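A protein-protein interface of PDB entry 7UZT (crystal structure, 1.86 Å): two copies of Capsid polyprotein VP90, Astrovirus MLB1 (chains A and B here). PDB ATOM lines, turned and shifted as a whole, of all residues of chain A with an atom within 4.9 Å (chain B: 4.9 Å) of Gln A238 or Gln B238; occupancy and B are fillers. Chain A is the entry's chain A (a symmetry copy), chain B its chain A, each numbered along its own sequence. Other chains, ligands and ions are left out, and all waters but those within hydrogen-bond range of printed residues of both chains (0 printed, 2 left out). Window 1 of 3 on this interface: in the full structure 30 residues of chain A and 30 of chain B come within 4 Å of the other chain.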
ATOM      1  N   LEU A 236       8.400 -31.901 -13.847  1.00  0.00           N
ATOM      2  CA  LEU A 236       9.625 -32.210 -14.557  1.00  0.00           C
ATOM      3  C   LEU A 236      10.340 -30.935 -14.979  1.00  0.00           C
ATOM      4  O   LEU A 236      11.383 -31.005 -15.631  1.00  0.00           O
ATOM      5  CB  LEU A 236       9.328 -33.115 -15.764  1.00  0.00           C
ATOM      6  CG  LEU A 236       8.989 -34.600 -15.437  1.00  0.00           C
ATOM      7  CD1 LEU A 236      10.188 -35.369 -15.066  1.00  0.00           C
ATOM      8  CD2 LEU A 236       7.899 -34.767 -14.370  1.00  0.00           C
ATOM      9  N   SER A 237       9.819 -29.775 -14.600  1.00  0.00           N
ATOM     10  CA  SER A 237      10.420 -28.508 -14.991  1.00  0.00           C
ATOM     11  C   SER A 237      11.323 -28.052 -13.854  1.00  0.00           C
ATOM     12  O   SER A 237      11.111 -28.417 -12.684  1.00  0.00           O
ATOM     13  CB  SER A 237       9.352 -27.438 -15.248  1.00  0.00           C
ATOM     14  OG  SER A 237       8.701 -27.102 -14.040  1.00  0.00           O
ATOM     15  N   GLN A 238      12.323 -27.231 -14.182  1.00  0.00           N
ATOM     16  CA  GLN A 238      12.639 -26.791 -15.537  1.00  0.00           C
ATOM     17  C   GLN A 238      13.624 -27.732 -16.208  1.00  0.00           C
ATOM     18  O   GLN A 238      14.041 -27.495 -17.341  1.00  0.00           O
ATOM     19  CB  GLN A 238      13.223 -25.392 -15.517  1.00  0.00           C
ATOM     20  CG  GLN A 238      12.278 -24.330 -14.975  1.00  0.00           C
ATOM     21  CD  GLN A 238      11.209 -24.068 -15.956  1.00  0.00           C
ATOM     22  OE1 GLN A 238      11.468 -24.094 -17.154  1.00  0.00           O
ATOM     23  NE2 GLN A 238      10.002 -23.769 -15.480  1.00  0.00           N
ATOM     24  N   LEU A 239      13.953 -28.813 -15.506  1.00  0.00           N
ATOM     25  CA  LEU A 239      14.953 -29.776 -15.959  1.00  0.00           C
ATOM     26  C   LEU A 239      14.717 -30.221 -17.394  1.00  0.00           C
ATOM     27  O   LEU A 239      15.568 -30.033 -18.264  1.00  0.00           O
ATOM     28  CB  LEU A 239      14.941 -30.990 -15.033  1.00  0.00           C
ATOM     29  CG  LEU A 239      15.981 -32.042 -15.388  1.00  0.00           C
ATOM     30  CD1 LEU A 239      17.337 -31.434 -15.603  1.00  0.00           C
ATOM     31  CD2 LEU A 239      16.010 -33.126 -14.343  1.00  0.00           C
ATOM     32  N   TYR A 240      13.571 -30.843 -17.641  1.00  0.00           N
ATOM     33  CA  TYR A 240      13.176 -31.287 -18.958  1.00  0.00           C
ATOM     34  C   TYR A 240      12.441 -30.147 -19.644  1.00  0.00           C
ATOM     35  O   TYR A 240      11.668 -29.410 -19.021  1.00  0.00           O
ATOM     36  CB  TYR A 240      12.296 -32.521 -18.848  1.00  0.00           C
ATOM     37  CG  TYR A 240      13.045 -33.671 -18.237  1.00  0.00           C
ATOM     38  CD1 TYR A 240      13.898 -34.462 -19.000  1.00  0.00           C
ATOM     39  CD2 TYR A 240      13.002 -33.884 -16.878  1.00  0.00           C
ATOM     40  CE1 TYR A 240      14.612 -35.500 -18.423  1.00  0.00           C
ATOM     41  CE2 TYR A 240      13.688 -34.907 -16.304  1.00  0.00           C
ATOM     42  CZ  TYR A 240      14.492 -35.707 -17.076  1.00  0.00           C
ATOM     43  OH  TYR A 240      15.176 -36.712 -16.479  1.00  0.00           O
ATOM     44  N   GLY A 241      12.654 -30.043 -20.921  1.00  0.00           N
ATOM     45  CA  GLY A 241      12.560 -28.795 -21.619  1.00  0.00           C
ATOM     46  C   GLY A 241      13.588 -28.844 -22.722  1.00  0.00           C
ATOM     47  O   GLY A 241      13.995 -29.929 -23.132  1.00  0.00           O
ATOM     48  N   SER A 243      16.827 -27.703 -23.294  1.00  0.00           N
ATOM     49  CA  SER A 243      18.276 -27.707 -23.357  1.00  0.00           C
ATOM     50  C   SER A 243      18.878 -27.925 -21.990  1.00  0.00           C
ATOM     51  O   SER A 243      18.430 -27.341 -21.011  1.00  0.00           O
ATOM     52  CB  SER A 243      18.794 -26.378 -23.945  1.00  0.00           C
ATOM     53  OG  SER A 243      20.208 -26.363 -23.936  1.00  0.00           O
ATOM     54  N   SER A 246      22.117 -24.790 -21.258  1.00  0.00           N
ATOM     55  CA  SER A 246      21.951 -23.653 -20.373  1.00  0.00           C
ATOM     56  C   SER A 246      21.655 -24.157 -18.975  1.00  0.00           C
ATOM     57  O   SER A 246      21.109 -25.259 -18.818  1.00  0.00           O
ATOM     58  CB  SER A 246      20.784 -22.800 -20.832  1.00  0.00           C
ATOM     59  OG  SER A 246      19.701 -23.667 -21.064  1.00  0.00           O
ATOM     60  N   PRO A 247      21.935 -23.374 -17.929  1.00  0.00           N
ATOM     61  CA  PRO A 247      21.691 -23.883 -16.565  1.00  0.00           C
ATOM     62  C   PRO A 247      20.199 -24.069 -16.318  1.00  0.00           C
ATOM     63  O   PRO A 247      19.364 -23.384 -16.920  1.00  0.00           O
ATOM     64  CB  PRO A 247      22.256 -22.778 -15.659  1.00  0.00           C
ATOM     65  CG  PRO A 247      22.190 -21.541 -16.491  1.00  0.00           C
ATOM     66  CD  PRO A 247      22.380 -21.971 -17.919  1.00  0.00           C
ATOM     67  N   THR A 248      19.857 -25.020 -15.449  1.00  0.00           N
ATOM     68  CA  THR A 248      18.448 -25.244 -15.143  1.00  0.00           C
ATOM     69  C   THR A 248      18.344 -25.787 -13.722  1.00  0.00           C
ATOM     70  O   THR A 248      19.294 -25.707 -12.928  1.00  0.00           O
ATOM     71  CB  THR A 248      17.806 -26.128 -16.244  1.00  0.00           C
ATOM     72  OG1 THR A 248      16.408 -26.304 -16.004  1.00  0.00           O
ATOM     73  CG2 THR A 248      18.445 -27.489 -16.354  1.00  0.00           C
ATOM     74  N   TYR A 249      17.168 -26.290 -13.370  1.00  0.00           N
ATOM     75  CA  TYR A 249      17.008 -26.859 -12.041  1.00  0.00           C
ATOM     76  C   TYR A 249      15.960 -27.952 -12.093  1.00  0.00           C
ATOM     77  O   TYR A 249      15.057 -27.945 -12.938  1.00  0.00           O
ATOM     78  CB  TYR A 249      16.598 -25.811 -10.978  1.00  0.00           C
ATOM     79  CG  TYR A 249      15.234 -25.235 -11.193  1.00  0.00           C
ATOM     80  CD1 TYR A 249      14.084 -25.912 -10.781  1.00  0.00           C
ATOM     81  CD2 TYR A 249      15.088 -24.010 -11.830  1.00  0.00           C
ATOM     82  CE1 TYR A 249      12.843 -25.401 -11.012  1.00  0.00           C
ATOM     83  CE2 TYR A 249      13.844 -23.470 -12.046  1.00  0.00           C
ATOM     84  CZ  TYR A 249      12.723 -24.183 -11.630  1.00  0.00           C
ATOM     85  OH  TYR A 249      11.467 -23.672 -11.847  1.00  0.00           O
ATOM     86  N   LEU B 236      15.773 -20.582 -26.656  1.00  0.00           N
ATOM     87  CA  LEU B 236      14.460 -20.368 -26.080  1.00  0.00           C
ATOM     88  C   LEU B 236      14.386 -20.948 -24.676  1.00  0.00           C
ATOM     89  O   LEU B 236      13.329 -20.895 -24.046  1.00  0.00           O
ATOM     90  CB  LEU B 236      13.375 -20.962 -26.994  1.00  0.00           C
ATOM     91  CG  LEU B 236      13.075 -20.170 -28.302  1.00  0.00           C
ATOM     92  CD1 LEU B 236      12.289 -18.954 -28.039  1.00  0.00           C
ATOM     93  CD2 LEU B 236      14.326 -19.828 -29.120  1.00  0.00           C
ATOM     94  N   SER B 237      15.489 -21.478 -24.162  1.00  0.00           N
ATOM     95  CA  SER B 237      15.495 -22.086 -22.840  1.00  0.00           C
ATOM     96  C   SER B 237      15.980 -21.038 -21.849  1.00  0.00           C
ATOM     97  O   SER B 237      16.716 -20.105 -22.215  1.00  0.00           O
ATOM     98  CB  SER B 237      16.430 -23.301 -22.787  1.00  0.00           C
ATOM     99  OG  SER B 237      17.772 -22.887 -22.935  1.00  0.00           O
ATOM    100  N   GLN B 238      15.593 -21.194 -20.581  1.00  0.00           N
ATOM    101  CA  GLN B 238      14.709 -22.250 -20.097  1.00  0.00           C
ATOM    102  C   GLN B 238      13.254 -21.819 -20.147  1.00  0.00           C
ATOM    103  O   GLN B 238      12.367 -22.565 -19.734  1.00  0.00           O
ATOM    104  CB  GLN B 238      15.067 -22.628 -18.672  1.00  0.00           C
ATOM    105  CG  GLN B 238      16.470 -23.193 -18.511  1.00  0.00           C
ATOM    106  CD  GLN B 238      16.527 -24.552 -19.082  1.00  0.00           C
ATOM    107  OE1 GLN B 238      15.559 -25.295 -18.972  1.00  0.00           O
ATOM    108  NE2 GLN B 238      17.667 -24.924 -19.661  1.00  0.00           N
ATOM    109  N   LEU B 239      13.028 -20.626 -20.690  1.00  0.00           N
ATOM    110  CA  LEU B 239      11.702 -20.016 -20.738  1.00  0.00           C
ATOM    111  C   LEU B 239      10.648 -20.970 -21.281  1.00  0.00           C
ATOM    112  O   LEU B 239       9.674 -21.291 -20.601  1.00  0.00           O
ATOM    113  CB  LEU B 239      11.755 -18.759 -21.602  1.00  0.00           C
ATOM    114  CG  LEU B 239      10.430 -18.016 -21.683  1.00  0.00           C
ATOM    115  CD1 LEU B 239       9.818 -17.816 -20.327  1.00  0.00           C
ATOM    116  CD2 LEU B 239      10.602 -16.713 -22.420  1.00  0.00           C
ATOM    117  N   TYR B 240      10.822 -21.401 -22.523  1.00  0.00           N
ATOM    118  CA  TYR B 240       9.939 -22.344 -23.169  1.00  0.00           C
ATOM    119  C   TYR B 240      10.430 -23.748 -22.856  1.00  0.00           C
ATOM    120  O   TYR B 240      11.637 -24.015 -22.815  1.00  0.00           O
ATOM    121  CB  TYR B 240       9.914 -22.091 -24.667  1.00  0.00           C
ATOM    122  CG  TYR B 240       9.358 -20.731 -24.980  1.00  0.00           C
ATOM    123  CD1 TYR B 240       7.987 -20.503 -25.014  1.00  0.00           C
ATOM    124  CD2 TYR B 240      10.201 -19.651 -25.113  1.00  0.00           C
ATOM    125  CE1 TYR B 240       7.481 -19.238 -25.269  1.00  0.00           C
ATOM    126  CE2 TYR B 240       9.716 -18.409 -25.377  1.00  0.00           C
ATOM    127  CZ  TYR B 240       8.362 -18.206 -25.450  1.00  0.00           C
ATOM    128  OH  TYR B 240       7.903 -16.957 -25.701  1.00  0.00           O
ATOM    129  N   GLY B 241       9.495 -24.634 -22.686  1.00  0.00           N
ATOM    130  CA  GLY B 241       9.673 -25.792 -21.860  1.00  0.00           C
ATOM    131  C   GLY B 241       8.328 -26.086 -21.242  1.00  0.00           C
ATOM    132  O   GLY B 241       7.304 -25.671 -21.780  1.00  0.00           O
ATOM    133  N   SER B 243       6.680 -25.503 -18.232  1.00  0.00           N
ATOM    134  CA  SER B 243       5.825 -24.854 -17.256  1.00  0.00           C
ATOM    135  C   SER B 243       6.311 -23.457 -16.955  1.00  0.00           C
ATOM    136  O   SER B 243       7.504 -23.233 -16.791  1.00  0.00           O
ATOM    137  CB  SER B 243       5.775 -25.677 -15.952  1.00  0.00           C
ATOM    138  OG  SER B 243       4.998 -24.999 -14.982  1.00  0.00           O
ATOM    139  N   SER B 246       6.500 -22.875 -12.430  1.00  0.00           N
ATOM    140  CA  SER B 246       7.737 -22.851 -11.672  1.00  0.00           C
ATOM    141  C   SER B 246       8.608 -21.724 -12.188  1.00  0.00           C
ATOM    142  O   SER B 246       8.491 -21.340 -13.362  1.00  0.00           O
ATOM    143  CB  SER B 246       8.486 -24.157 -11.854  1.00  0.00           C
ATOM    144  OG  SER B 246       8.518 -24.429 -13.234  1.00  0.00           O
ATOM    145  N   PRO B 247       9.536 -21.198 -11.383  1.00  0.00           N
ATOM    146  CA  PRO B 247      10.352 -20.068 -11.868  1.00  0.00           C
ATOM    147  C   PRO B 247      11.262 -20.512 -13.006  1.00  0.00           C
ATOM    148  O   PRO B 247      11.649 -21.683 -13.092  1.00  0.00           O
ATOM    149  CB  PRO B 247      11.180 -19.663 -10.638  1.00  0.00           C
ATOM    150  CG  PRO B 247      11.245 -20.901  -9.808  1.00  0.00           C
ATOM    151  CD  PRO B 247       9.965 -21.652 -10.050  1.00  0.00           C
ATOM    152  N   THR B 248      11.587 -19.580 -13.902  1.00  0.00           N
ATOM    153  CA  THR B 248      12.474 -19.923 -15.010  1.00  0.00           C
ATOM    154  C   THR B 248      13.235 -18.668 -15.423  1.00  0.00           C
ATOM    155  O   THR B 248      13.281 -17.667 -14.690  1.00  0.00           O
ATOM    156  CB  THR B 248      11.663 -20.613 -16.137  1.00  0.00           C
ATOM    157  OG1 THR B 248      12.522 -21.022 -17.204  1.00  0.00           O
ATOM    158  CG2 THR B 248      10.580 -19.734 -16.708  1.00  0.00           C
ATOM    159  N   TYR B 249      13.889 -18.731 -16.576  1.00  0.00           N
ATOM    160  CA  TYR B 249      14.606 -17.557 -17.050  1.00  0.00           C
ATOM    161  C   TYR B 249      14.633 -17.572 -18.565  1.00  0.00           C
ATOM    162  O   TYR B 249      14.567 -18.628 -19.205  1.00  0.00           O
ATOM    163  CB  TYR B 249      16.057 -17.476 -16.517  1.00  0.00           C
ATOM    164  CG  TYR B 249      16.948 -18.564 -17.026  1.00  0.00           C
ATOM    165  CD1 TYR B 249      17.545 -18.487 -18.287  1.00  0.00           C
ATOM    166  CD2 TYR B 249      17.185 -19.691 -16.250  1.00  0.00           C
ATOM    167  CE1 TYR B 249      18.326 -19.497 -18.761  1.00  0.00           C
ATOM    168  CE2 TYR B 249      17.992 -20.706 -16.705  1.00  0.00           C
ATOM    169  CZ  TYR B 249      18.558 -20.594 -17.971  1.00  0.00           C
ATOM    170  OH  TYR B 249      19.357 -21.600 -18.456  1.00  0.00           O
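The side-chain hydroxyl (OG) of Ser A246 sits at hydrogen-bond distance from the side-chain hydroxyl (OG) of Ser B237.
The backbone carbonyl oxygen of Gln B238 sits close to the side-chain amide oxygen of Gln A238 (3.1 Å).
NE2 of Gln B238 is in hydrogen-bond range of O of Ser A243, at 2.9 Å.
NE2 of Gln B238 lies within hydrogen-bond range of OG of Ser A246 (2.8 Å).
The side-chain amide oxygen (OE1) of Gln B238 is in hydrogen-bond range of the side-chain hydroxyl (OG1) of Thr A248 (3.2 Å).
The backbone carbonyl oxygen (O) of Ser B243 lies within hydrogen-bond range of the side-chain amide nitrogen (NE2) of Gln A238 (2.9 Å).
The side-chain hydroxyl (OG) of Ser B246 sits at hydrogen-bond distance from the side-chain hydroxyl (OG) of Ser A237 (2.8 Å).
NE2 of Gln A238 lies within hydrogen-bond range of OG of Ser B246 (2.8 Å).
The side-chain hydroxyl (OH) of Tyr A249 lies close to the side-chain hydroxyl (OG) of Ser B246 (3.3 Å).
The side-chain amide oxygen (OE1) of Gln A238 is in hydrogen-bond range of the side-chain hydroxyl (OG1) of Thr B248 (3.2 Å).
The side-chain hydroxyl (OH) of Tyr B249 sits close to the side-chain hydroxyl (OG) of Ser A246, at 3.3 Å.
O of Pro A247 lies close to OH of Tyr B249.
OH of Tyr A249 lies close to O of Pro B247, at 2.4 Å.
The backbone carbonyl oxygen (O) of Gln B238 sits at hydrogen-bond distance from the side-chain hydroxyl (OG1) of Thr B248 (3.0 Å).
The backbone carbonyl oxygen of Tyr B249 sits at hydrogen-bond distance from the backbone NH of Gln B238 (3.1 Å).
The backbone NH (N) of Leu B239 is in hydrogen-bond range of the backbone carbonyl oxygen (O) of Tyr B249 (2.9 Å).
OG1 of Thr A248 is in hydrogen-bond range of O of Gln A238, 3.0 Å away.
The backbone NH (N) of Gln A238 sits at hydrogen-bond distance from the backbone carbonyl oxygen (O) of Tyr A249 (3.1 Å).
The backbone NH (N) of Leu A239 sits at hydrogen-bond distance from the backbone carbonyl oxygen (O) of Tyr A249 (2.9 Å).
Ser A237 touches Ser B243 (OG to CB, 3.8 Å).
Gln A238 touches Pro B247.
Ser A243 touches Ser B237 (CB to OG, 3.8 Å).
O of Pro A247 touches CG of Gln B238, at 3.3 Å.
Gln A238 touches just these residues of chain B: Gln B238, Ser B243, Ser B246, Pro B247 and Thr B248.
Gln B238 touches five residues of chain A.
Printed residues of chain A within 4 Å of Thr B248: Gln A238.
Printed residues of chain A within 4 Å of Ser B243: Ser A237 (3.8 Å) and Gln A238 (2.9 Å).
Printed residues of chain B within 4 Å of Ser A237: Ser B243 and Ser B246.
The nearest residue of chain A that does not touch Gln B238 is Leu A239 (4.8 Å).
Hydrophobic or aromatic side chains of chain A that line the printed part of chain B: Pro A247 and Tyr A249.
Hydrophobic or aromatic side chains of chain B within 4 Å of the printed part of chain A: Pro B247 and Tyr B249.
Along chain B the printed residues that touch a printed residue of chain A span positions 237 to 249.
Ser A237 touches Ser B243, and with the chains exchanged Ser A243 touches Ser B237.
Ser A237 touches Ser B246, and with the chains exchanged Ser A246 touches Ser B237.
Ser A246 touches Tyr B249, and with the chains exchanged Tyr A249 touches Ser B246.
Pro A247 touches Tyr B249, and with the chains exchanged Tyr A249 touches Pro B247.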
